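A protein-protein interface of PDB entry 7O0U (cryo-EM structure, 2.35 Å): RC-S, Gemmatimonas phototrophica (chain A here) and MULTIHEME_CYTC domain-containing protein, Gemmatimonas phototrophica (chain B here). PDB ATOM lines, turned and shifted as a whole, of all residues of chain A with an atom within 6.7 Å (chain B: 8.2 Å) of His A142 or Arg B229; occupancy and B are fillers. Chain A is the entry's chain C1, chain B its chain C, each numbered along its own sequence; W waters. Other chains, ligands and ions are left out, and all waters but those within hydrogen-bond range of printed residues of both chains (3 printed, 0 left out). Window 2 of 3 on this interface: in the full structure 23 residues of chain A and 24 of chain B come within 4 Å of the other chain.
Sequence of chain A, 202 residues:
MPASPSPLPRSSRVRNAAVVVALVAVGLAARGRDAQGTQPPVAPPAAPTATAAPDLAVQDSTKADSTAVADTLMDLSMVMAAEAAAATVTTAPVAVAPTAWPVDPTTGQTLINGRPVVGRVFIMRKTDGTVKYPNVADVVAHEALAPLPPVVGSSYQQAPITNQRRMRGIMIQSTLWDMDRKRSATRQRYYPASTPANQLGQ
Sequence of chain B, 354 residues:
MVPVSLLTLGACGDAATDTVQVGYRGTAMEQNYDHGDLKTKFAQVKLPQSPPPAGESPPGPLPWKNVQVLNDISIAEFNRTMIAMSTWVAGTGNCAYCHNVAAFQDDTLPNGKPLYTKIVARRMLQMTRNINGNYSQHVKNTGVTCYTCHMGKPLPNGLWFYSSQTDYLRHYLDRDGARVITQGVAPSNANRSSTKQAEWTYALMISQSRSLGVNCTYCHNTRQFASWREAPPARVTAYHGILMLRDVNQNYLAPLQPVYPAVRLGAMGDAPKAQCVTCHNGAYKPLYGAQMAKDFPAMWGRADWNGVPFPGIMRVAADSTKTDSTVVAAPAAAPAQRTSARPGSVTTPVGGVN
OD1 of Asn B221 sits close to N of Arg B223, 3.3 Å away. OE2 of Glu B230 lies within salt-bridge range of NH2 of Arg B223 (2.7 Å). The guanidinium group (NH1) of Arg B235 sits at hydrogen-bond distance from the backbone carbonyl oxygen (O) of Ala B226 (3.1 Å). The backbone NH (N) of Glu B230 is in hydrogen-bond range of the side-chain hydroxyl (OG) of Ser B227. The backbone carbonyl oxygen (O) of Ser B227 is in hydrogen-bond range of the guanidinium group (NH1) of Arg B235. A ring nitrogen (ND1) of His A142 is in hydrogen-bond range of the backbone carbonyl oxygen of Asp A138, at 2.7 Å.
Water W2 bridges the side-chain carboxylate of Asp A138 and the guanidinium group of Arg B229. Water W1 lies within hydrogen-bond range of the backbone carbonyl oxygen of Ala B226 (2.6 Å) and the side-chain carboxylate of Glu A143 (2.7 Å). Water W3 lies within hydrogen-bond range of OE2 of Glu A143 (2.6 Å) and NE of Arg B229 (3.1 Å).
Hydrophobic or aromatic side chains of chain B that line the printed part of chain A: Trp B228. Hydrophobic or aromatic side chains of chain A that line the printed part of chain B: Tyr A133, Val A139, Val A140, His A142 and Ala A144. Along chain A the printed residues that touch a printed residue of chain B span positions 133 to 144. Among the printed residues, 12 pairs touch across the chains.
Of the printed residues of chain B, Tyr A133 touches Arg B223 (3.2 Å), Arg B229 (3.7 Å) and Glu B230 (3.1 Å). Of the printed residues of chain B, Val A139 touches Arg B229 (3.9 Å). No residue of chain B comes within 4 Å of Ala A141. Of chain B, only Arg B229 comes within 4 Å of His A142. Printed residues of chain A within 4 Å of Gln B183: Val A140 and Ala A144. Printed residues of chain A within 4 Å of Ser B227: Glu A143. Arg B229 touches just these residues of chain A: Tyr A133 (3.7 Å), Val A139 (3.9 Å), His A142 (3.6 Å) and Glu A143 (3.5 Å).
Arg B229 touches Tyr A133. Arg B229 touches Val A139 (NH2 to CG2, 3.9 Å). Val A140 touches Gln B183 (CG1 to OE1, 3.9 Å). His A142 touches Arg B229. OE1 of Glu A143 touches O of Ala B226, 3.9 Å away. Arg B229 touches Glu A143 (N to OE2, 3.5 Å). CB of Ala A144 touches CD1 of Trp B228, at 3.9 Å.
NE2 of Gln B183 is in hydrogen-bond range of O of Ala A144, 2.9 Å away. NH2 of Arg B223 is in hydrogen-bond range of OH of Tyr A133 (3.2 Å). The side-chain hydroxyl (OG) of Ser B227 lies within hydrogen-bond range of the side-chain carboxylate (OE2) of Glu A143, at 2.7 Å. OE1 of Glu A143 is in hydrogen-bond range of N of Trp B228. OE2 of Glu B230 lies within hydrogen-bond range of OH of Tyr A133, 3.1 Å away.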
ATOM      1  N   TYR A 133      16.693  23.441  26.552  1.00  0.00           N
ATOM      2  CA  TYR A 133      16.409  22.895  25.223  1.00  0.00           C
ATOM      3  C   TYR A 133      14.942  22.491  25.116  1.00  0.00           C
ATOM      4  O   TYR A 133      14.443  21.761  25.981  1.00  0.00           O
ATOM      5  CB  TYR A 133      17.284  21.676  24.918  1.00  0.00           C
ATOM      6  CG  TYR A 133      18.783  21.894  24.893  1.00  0.00           C
ATOM      7  CD1 TYR A 133      19.330  23.151  24.676  1.00  0.00           C
ATOM      8  CD2 TYR A 133      19.651  20.821  25.045  1.00  0.00           C
ATOM      9  CE1 TYR A 133      20.704  23.340  24.675  1.00  0.00           C
ATOM     10  CE2 TYR A 133      21.019  20.995  25.012  1.00  0.00           C
ATOM     11  CZ  TYR A 133      21.542  22.255  24.837  1.00  0.00           C
ATOM     12  OH  TYR A 133      22.905  22.419  24.773  1.00  0.00           O
ATOM     13  N   PRO A 134      14.221  22.936  24.082  1.00  0.00           N
ATOM     14  CA  PRO A 134      12.770  22.700  24.032  1.00  0.00           C
ATOM     15  C   PRO A 134      12.414  21.239  23.800  1.00  0.00           C
ATOM     16  O   PRO A 134      11.546  20.689  24.484  1.00  0.00           O
ATOM     17  CB  PRO A 134      12.309  23.577  22.858  1.00  0.00           C
ATOM     18  CG  PRO A 134      13.378  24.603  22.701  1.00  0.00           C
ATOM     19  CD  PRO A 134      14.652  23.889  23.050  1.00  0.00           C
ATOM     20  N   ALA A 137      13.569  17.965  18.313  1.00  0.00           N
ATOM     21  CA  ALA A 137      13.493  18.592  16.996  1.00  0.00           C
ATOM     22  C   ALA A 137      14.217  19.934  16.956  1.00  0.00           C
ATOM     23  O   ALA A 137      14.879  20.260  15.965  1.00  0.00           O
ATOM     24  CB  ALA A 137      12.031  18.761  16.582  1.00  0.00           C
ATOM     25  N   ASP A 138      14.109  20.720  18.026  1.00  0.00           N
ATOM     26  CA  ASP A 138      14.825  21.991  18.094  1.00  0.00           C
ATOM     27  C   ASP A 138      16.334  21.803  18.209  1.00  0.00           C
ATOM     28  O   ASP A 138      17.103  22.538  17.580  1.00  0.00           O
ATOM     29  CB  ASP A 138      14.307  22.819  19.266  1.00  0.00           C
ATOM     30  CG  ASP A 138      14.940  24.190  19.326  1.00  0.00           C
ATOM     31  OD1 ASP A 138      14.515  25.075  18.556  1.00  0.00           O
ATOM     32  OD2 ASP A 138      15.871  24.382  20.136  1.00  0.00           O
ATOM     33  N   VAL A 139      16.776  20.832  19.009  1.00  0.00           N
ATOM     34  CA  VAL A 139      18.195  20.478  19.052  1.00  0.00           C
ATOM     35  C   VAL A 139      18.695  20.051  17.675  1.00  0.00           C
ATOM     36  O   VAL A 139      19.736  20.521  17.203  1.00  0.00           O
ATOM     37  CB  VAL A 139      18.436  19.381  20.106  1.00  0.00           C
ATOM     38  CG1 VAL A 139      19.831  18.796  19.964  1.00  0.00           C
ATOM     39  CG2 VAL A 139      18.233  19.944  21.503  1.00  0.00           C
ATOM     40  N   VAL A 140      17.960  19.158  17.011  1.00  0.00           N
ATOM     41  CA  VAL A 140      18.350  18.685  15.683  1.00  0.00           C
ATOM     42  C   VAL A 140      18.325  19.800  14.639  1.00  0.00           C
ATOM     43  O   VAL A 140      19.153  19.812  13.719  1.00  0.00           O
ATOM     44  CB  VAL A 140      17.451  17.498  15.274  1.00  0.00           C
ATOM     45  CG1 VAL A 140      17.653  17.133  13.813  1.00  0.00           C
ATOM     46  CG2 VAL A 140      17.744  16.296  16.155  1.00  0.00           C
ATOM     47  N   ALA A 141      17.412  20.764  14.769  1.00  0.00           N
ATOM     48  CA  ALA A 141      17.379  21.885  13.832  1.00  0.00           C
ATOM     49  C   ALA A 141      18.601  22.796  13.915  1.00  0.00           C
ATOM     50  O   ALA A 141      18.845  23.559  12.974  1.00  0.00           O
ATOM     51  CB  ALA A 141      16.112  22.712  14.055  1.00  0.00           C
ATOM     52  N   HIS A 142      19.366  22.749  15.001  1.00  0.00           N
ATOM     53  CA  HIS A 142      20.617  23.496  15.074  1.00  0.00           C
ATOM     54  C   HIS A 142      21.815  22.729  14.528  1.00  0.00           C
ATOM     55  O   HIS A 142      22.872  23.332  14.320  1.00  0.00           O
ATOM     56  CB  HIS A 142      20.891  23.943  16.513  1.00  0.00           C
ATOM     57  CG  HIS A 142      19.961  25.014  16.991  1.00  0.00           C
ATOM     58  ND1 HIS A 142      18.736  24.745  17.562  1.00  0.00           N
ATOM     59  CD2 HIS A 142      20.072  26.363  16.960  1.00  0.00           C
ATOM     60  CE1 HIS A 142      18.138  25.881  17.872  1.00  0.00           C
ATOM     61  NE2 HIS A 142      18.928  26.878  17.517  1.00  0.00           N
ATOM     62  N   GLU A 143      21.680  21.428  14.301  1.00  0.00           N
ATOM     63  CA  GLU A 143      22.776  20.595  13.834  1.00  0.00           C
ATOM     64  C   GLU A 143      22.850  20.598  12.307  1.00  0.00           C
ATOM     65  O   GLU A 143      21.977  21.129  11.617  1.00  0.00           O
ATOM     66  CB  GLU A 143      22.613  19.172  14.364  1.00  0.00           C
ATOM     67  CG  GLU A 143      22.796  19.056  15.869  1.00  0.00           C
ATOM     68  CD  GLU A 143      24.154  19.539  16.339  1.00  0.00           C
ATOM     69  OE1 GLU A 143      25.123  19.462  15.555  1.00  0.00           O
ATOM     70  OE2 GLU A 143      24.254  20.002  17.493  1.00  0.00           O
ATOM     71  N   ALA A 144      23.921  20.008  11.780  1.00  0.00           N
ATOM     72  CA  ALA A 144      23.967  19.678  10.363  1.00  0.00           C
ATOM     73  C   ALA A 144      22.831  18.727   9.993  1.00  0.00           C
ATOM     74  O   ALA A 144      22.246  18.052  10.844  1.00  0.00           O
ATOM     75  CB  ALA A 144      25.315  19.054  10.004  1.00  0.00           C
ATOM     76  N   MET B  29      36.112  21.083  28.918  1.00  0.00           N
ATOM     77  CA  MET B  29      36.693  21.128  27.576  1.00  0.00           C
ATOM     78  C   MET B  29      37.968  21.965  27.646  1.00  0.00           C
ATOM     79  O   MET B  29      37.945  23.191  27.534  1.00  0.00           O
ATOM     80  CB  MET B  29      35.677  21.653  26.571  1.00  0.00           C
ATOM     81  CG  MET B  29      34.523  20.671  26.377  1.00  0.00           C
ATOM     82  SD  MET B  29      33.128  21.260  25.401  1.00  0.00           S
ATOM     83  CE  MET B  29      33.956  21.784  23.906  1.00  0.00           C
ATOM     84  N   GLN B 183      20.966  10.364  14.215  1.00  0.00           N
ATOM     85  CA  GLN B 183      20.376  11.678  14.477  1.00  0.00           C
ATOM     86  C   GLN B 183      18.880  11.545  14.776  1.00  0.00           C
ATOM     87  O   GLN B 183      18.017  12.131  14.124  1.00  0.00           O
ATOM     88  CB  GLN B 183      20.652  12.622  13.310  1.00  0.00           C
ATOM     89  CG  GLN B 183      20.367  14.087  13.611  1.00  0.00           C
ATOM     90  CD  GLN B 183      20.651  14.996  12.433  1.00  0.00           C
ATOM     91  OE1 GLN B 183      19.890  15.042  11.469  1.00  0.00           O
ATOM     92  NE2 GLN B 183      21.755  15.730  12.509  1.00  0.00           N
ATOM     93  N   ASN B 221      32.255  18.425  22.069  1.00  0.00           N
ATOM     94  CA  ASN B 221      31.766  18.186  23.421  1.00  0.00           C
ATOM     95  C   ASN B 221      31.436  16.698  23.463  1.00  0.00           C
ATOM     96  O   ASN B 221      30.499  16.246  22.798  1.00  0.00           O
ATOM     97  CB  ASN B 221      30.556  19.057  23.751  1.00  0.00           C
ATOM     98  CG  ASN B 221      30.137  18.957  25.209  1.00  0.00           C
ATOM     99  OD1 ASN B 221      30.336  17.935  25.860  1.00  0.00           O
ATOM    100  ND2 ASN B 221      29.560  20.030  25.729  1.00  0.00           N
ATOM    101  N   ARG B 223      29.995  14.704  25.399  1.00  0.00           N
ATOM    102  CA  ARG B 223      28.647  14.239  25.704  1.00  0.00           C
ATOM    103  C   ARG B 223      27.825  13.960  24.450  1.00  0.00           C
ATOM    104  O   ARG B 223      26.849  13.206  24.521  1.00  0.00           O
ATOM    105  CB  ARG B 223      27.937  15.239  26.619  1.00  0.00           C
ATOM    106  CG  ARG B 223      27.252  16.397  25.934  1.00  0.00           C
ATOM    107  CD  ARG B 223      26.575  17.266  26.977  1.00  0.00           C
ATOM    108  NE  ARG B 223      25.818  18.362  26.392  1.00  0.00           N
ATOM    109  CZ  ARG B 223      24.934  19.095  27.055  1.00  0.00           C
ATOM    110  NH1 ARG B 223      24.681  18.883  28.335  1.00  0.00           N
ATOM    111  NH2 ARG B 223      24.293  20.070  26.418  1.00  0.00           N
ATOM    112  N   GLN B 224      28.190  14.550  23.311  1.00  0.00           N
ATOM    113  CA  GLN B 224      27.580  14.205  22.026  1.00  0.00           C
ATOM    114  C   GLN B 224      28.586  14.523  20.923  1.00  0.00           C
ATOM    115  O   GLN B 224      28.676  15.671  20.480  1.00  0.00           O
ATOM    116  CB  GLN B 224      26.271  14.962  21.828  1.00  0.00           C
ATOM    117  CG  GLN B 224      25.504  14.656  20.536  1.00  0.00           C
ATOM    118  CD  GLN B 224      24.957  13.235  20.414  1.00  0.00           C
ATOM    119  OE1 GLN B 224      24.297  12.914  19.427  1.00  0.00           O
ATOM    120  NE2 GLN B 224      25.187  12.401  21.421  1.00  0.00           N
ATOM    121  N   PHE B 225      29.340  13.509  20.491  1.00  0.00           N
ATOM    122  CA  PHE B 225      30.365  13.728  19.472  1.00  0.00           C
ATOM    123  C   PHE B 225      29.780  14.249  18.163  1.00  0.00           C
ATOM    124  O   PHE B 225      30.439  15.018  17.455  1.00  0.00           O
ATOM    125  CB  PHE B 225      31.153  12.443  19.218  1.00  0.00           C
ATOM    126  CG  PHE B 225      32.138  12.104  20.301  1.00  0.00           C
ATOM    127  CD1 PHE B 225      33.375  12.724  20.342  1.00  0.00           C
ATOM    128  CD2 PHE B 225      31.841  11.152  21.262  1.00  0.00           C
ATOM    129  CE1 PHE B 225      34.291  12.412  21.325  1.00  0.00           C
ATOM    130  CE2 PHE B 225      32.754  10.838  22.251  1.00  0.00           C
ATOM    131  CZ  PHE B 225      33.981  11.467  22.280  1.00  0.00           C
ATOM    132  N   ALA B 226      28.557  13.840  17.822  1.00  0.00           N
ATOM    133  CA  ALA B 226      27.909  14.302  16.597  1.00  0.00           C
ATOM    134  C   ALA B 226      27.592  15.795  16.587  1.00  0.00           C
ATOM    135  O   ALA B 226      27.457  16.368  15.502  1.00  0.00           O
ATOM    136  CB  ALA B 226      26.623  13.512  16.363  1.00  0.00           C
ATOM    137  N   SER B 227      27.468  16.436  17.746  1.00  0.00           N
ATOM    138  CA  SER B 227      26.975  17.810  17.786  1.00  0.00           C
ATOM    139  C   SER B 227      28.010  18.795  17.251  1.00  0.00           C
ATOM    140  O   SER B 227      29.186  18.744  17.622  1.00  0.00           O
ATOM    141  CB  SER B 227      26.585  18.190  19.210  1.00  0.00           C
ATOM    142  OG  SER B 227      26.200  19.551  19.277  1.00  0.00           O
ATOM    143  N   TRP B 228      27.558  19.698  16.377  1.00  0.00           N
ATOM    144  CA  TRP B 228      28.334  20.845  15.920  1.00  0.00           C
ATOM    145  C   TRP B 228      28.127  22.091  16.776  1.00  0.00           C
ATOM    146  O   TRP B 228      29.079  22.841  17.013  1.00  0.00           O
ATOM    147  CB  TRP B 228      27.992  21.158  14.463  1.00  0.00           C
ATOM    148  CG  TRP B 228      28.428  20.084  13.525  1.00  0.00           C
ATOM    149  CD1 TRP B 228      27.703  18.999  13.137  1.00  0.00           C
ATOM    150  CD2 TRP B 228      29.693  19.981  12.863  1.00  0.00           C
ATOM    151  NE1 TRP B 228      28.434  18.226  12.272  1.00  0.00           N
ATOM    152  CE2 TRP B 228      29.662  18.806  12.089  1.00  0.00           C
ATOM    153  CE3 TRP B 228      30.849  20.765  12.851  1.00  0.00           C
ATOM    154  CZ2 TRP B 228      30.739  18.398  11.307  1.00  0.00           C
ATOM    155  CZ3 TRP B 228      31.918  20.359  12.075  1.00  0.00           C
ATOM    156  CH2 TRP B 228      31.856  19.187  11.314  1.00  0.00           C
ATOM    157  N   ARG B 229      26.896  22.333  17.235  1.00  0.00           N
ATOM    158  CA  ARG B 229      26.624  23.509  18.059  1.00  0.00           C
ATOM    159  C   ARG B 229      27.409  23.475  19.364  1.00  0.00           C
ATOM    160  O   ARG B 229      27.936  24.502  19.807  1.00  0.00           O
ATOM    161  CB  ARG B 229      25.125  23.619  18.348  1.00  0.00           C
ATOM    162  CG  ARG B 229      24.783  24.719  19.343  1.00  0.00           C
ATOM    163  CD  ARG B 229      23.291  25.007  19.417  1.00  0.00           C
ATOM    164  NE  ARG B 229      22.535  23.896  19.980  1.00  0.00           N
ATOM    165  CZ  ARG B 229      21.329  24.011  20.521  1.00  0.00           C
ATOM    166  NH1 ARG B 229      20.712  25.179  20.592  1.00  0.00           N
ATOM    167  NH2 ARG B 229      20.729  22.928  21.004  1.00  0.00           N
ATOM    168  N   GLU B 230      27.504  22.305  19.989  1.00  0.00           N
ATOM    169  CA  GLU B 230      28.220  22.178  21.250  1.00  0.00           C
ATOM    170  C   GLU B 230      29.730  22.102  21.061  1.00  0.00           C
ATOM    171  O   GLU B 230      30.474  22.324  22.021  1.00  0.00           O
ATOM    172  CB  GLU B 230      27.704  20.949  22.002  1.00  0.00           C
ATOM    173  CG  GLU B 230      26.237  21.074  22.389  1.00  0.00           C
ATOM    174  CD  GLU B 230      25.774  20.002  23.354  1.00  0.00           C
ATOM    175  OE1 GLU B 230      26.576  19.109  23.690  1.00  0.00           O
ATOM    176  OE2 GLU B 230      24.602  20.055  23.779  1.00  0.00           O
ATOM    177  N   ALA B 231      30.194  21.788  19.856  1.00  0.00           N
ATOM    178  CA  ALA B 231      31.611  21.699  19.545  1.00  0.00           C
ATOM    179  C   ALA B 231      32.203  23.087  19.300  1.00  0.00           C
ATOM    180  O   ALA B 231      31.508  23.991  18.832  1.00  0.00           O
ATOM    181  CB  ALA B 231      31.822  20.829  18.313  1.00  0.00           C
ATOM    182  N   PRO B 232      33.483  23.282  19.613  1.00  0.00           N
ATOM    183  CA  PRO B 232      34.170  24.520  19.219  1.00  0.00           C
ATOM    184  C   PRO B 232      34.168  24.710  17.712  1.00  0.00           C
ATOM    185  O   PRO B 232      33.962  23.751  16.952  1.00  0.00           O
ATOM    186  CB  PRO B 232      35.596  24.318  19.761  1.00  0.00           C
ATOM    187  CG  PRO B 232      35.436  23.305  20.850  1.00  0.00           C
ATOM    188  CD  PRO B 232      34.394  22.370  20.318  1.00  0.00           C
ATOM    189  N   PRO B 233      34.403  25.939  17.243  1.00  0.00           N
ATOM    190  CA  PRO B 233      34.485  26.182  15.793  1.00  0.00           C
ATOM    191  C   PRO B 233      35.611  25.440  15.090  1.00  0.00           C
ATOM    192  O   PRO B 233      35.515  25.198  13.880  1.00  0.00           O
ATOM    193  CB  PRO B 233      34.684  27.704  15.709  1.00  0.00           C
ATOM    194  CG  PRO B 233      34.113  28.226  16.980  1.00  0.00           C
ATOM    195  CD  PRO B 233      34.479  27.193  18.005  1.00  0.00           C
ATOM    196  N   ARG B 235      36.245  22.424  14.973  1.00  0.00           N
ATOM    197  CA  ARG B 235      35.740  21.237  14.285  1.00  0.00           C
ATOM    198  C   ARG B 235      35.396  21.520  12.826  1.00  0.00           C
ATOM    199  O   ARG B 235      35.589  20.658  11.961  1.00  0.00           O
ATOM    200  CB  ARG B 235      34.519  20.671  15.006  1.00  0.00           C
ATOM    201  CG  ARG B 235      34.232  19.236  14.595  1.00  0.00           C
ATOM    202  CD  ARG B 235      32.950  18.687  15.182  1.00  0.00           C
ATOM    203  NE  ARG B 235      32.686  17.350  14.665  1.00  0.00           N
ATOM    204  CZ  ARG B 235      31.483  16.803  14.564  1.00  0.00           C
ATOM    205  NH1 ARG B 235      30.427  17.345  15.144  1.00  0.00           N
ATOM    206  NH2 ARG B 235      31.348  15.651  13.914  1.00  0.00           N
ATOM    207  N   VAL B 236      34.871  22.710  12.532  1.00  0.00           N
ATOM    208  CA  VAL B 236      34.551  23.057  11.149  1.00  0.00           C
ATOM    209  C   VAL B 236      35.818  23.189  10.312  1.00  0.00           C
ATOM    210  O   VAL B 236      35.882  22.692   9.182  1.00  0.00           O
ATOM    211  CB  VAL B 236      33.702  24.341  11.103  1.00  0.00           C
ATOM    212  CG1 VAL B 236      33.405  24.729   9.664  1.00  0.00           C
ATOM    213  CG2 VAL B 236      32.410  24.145  11.871  1.00  0.00           C
HETATM  214  O   HOH W   1      25.129  16.966  14.466  1.00  0.00           O
HETATM  215  O   HOH W   2      17.940  24.655  21.631  1.00  0.00           O
HETATM  216  O   HOH W   3      22.914  20.887  19.573  1.00  0.00           O
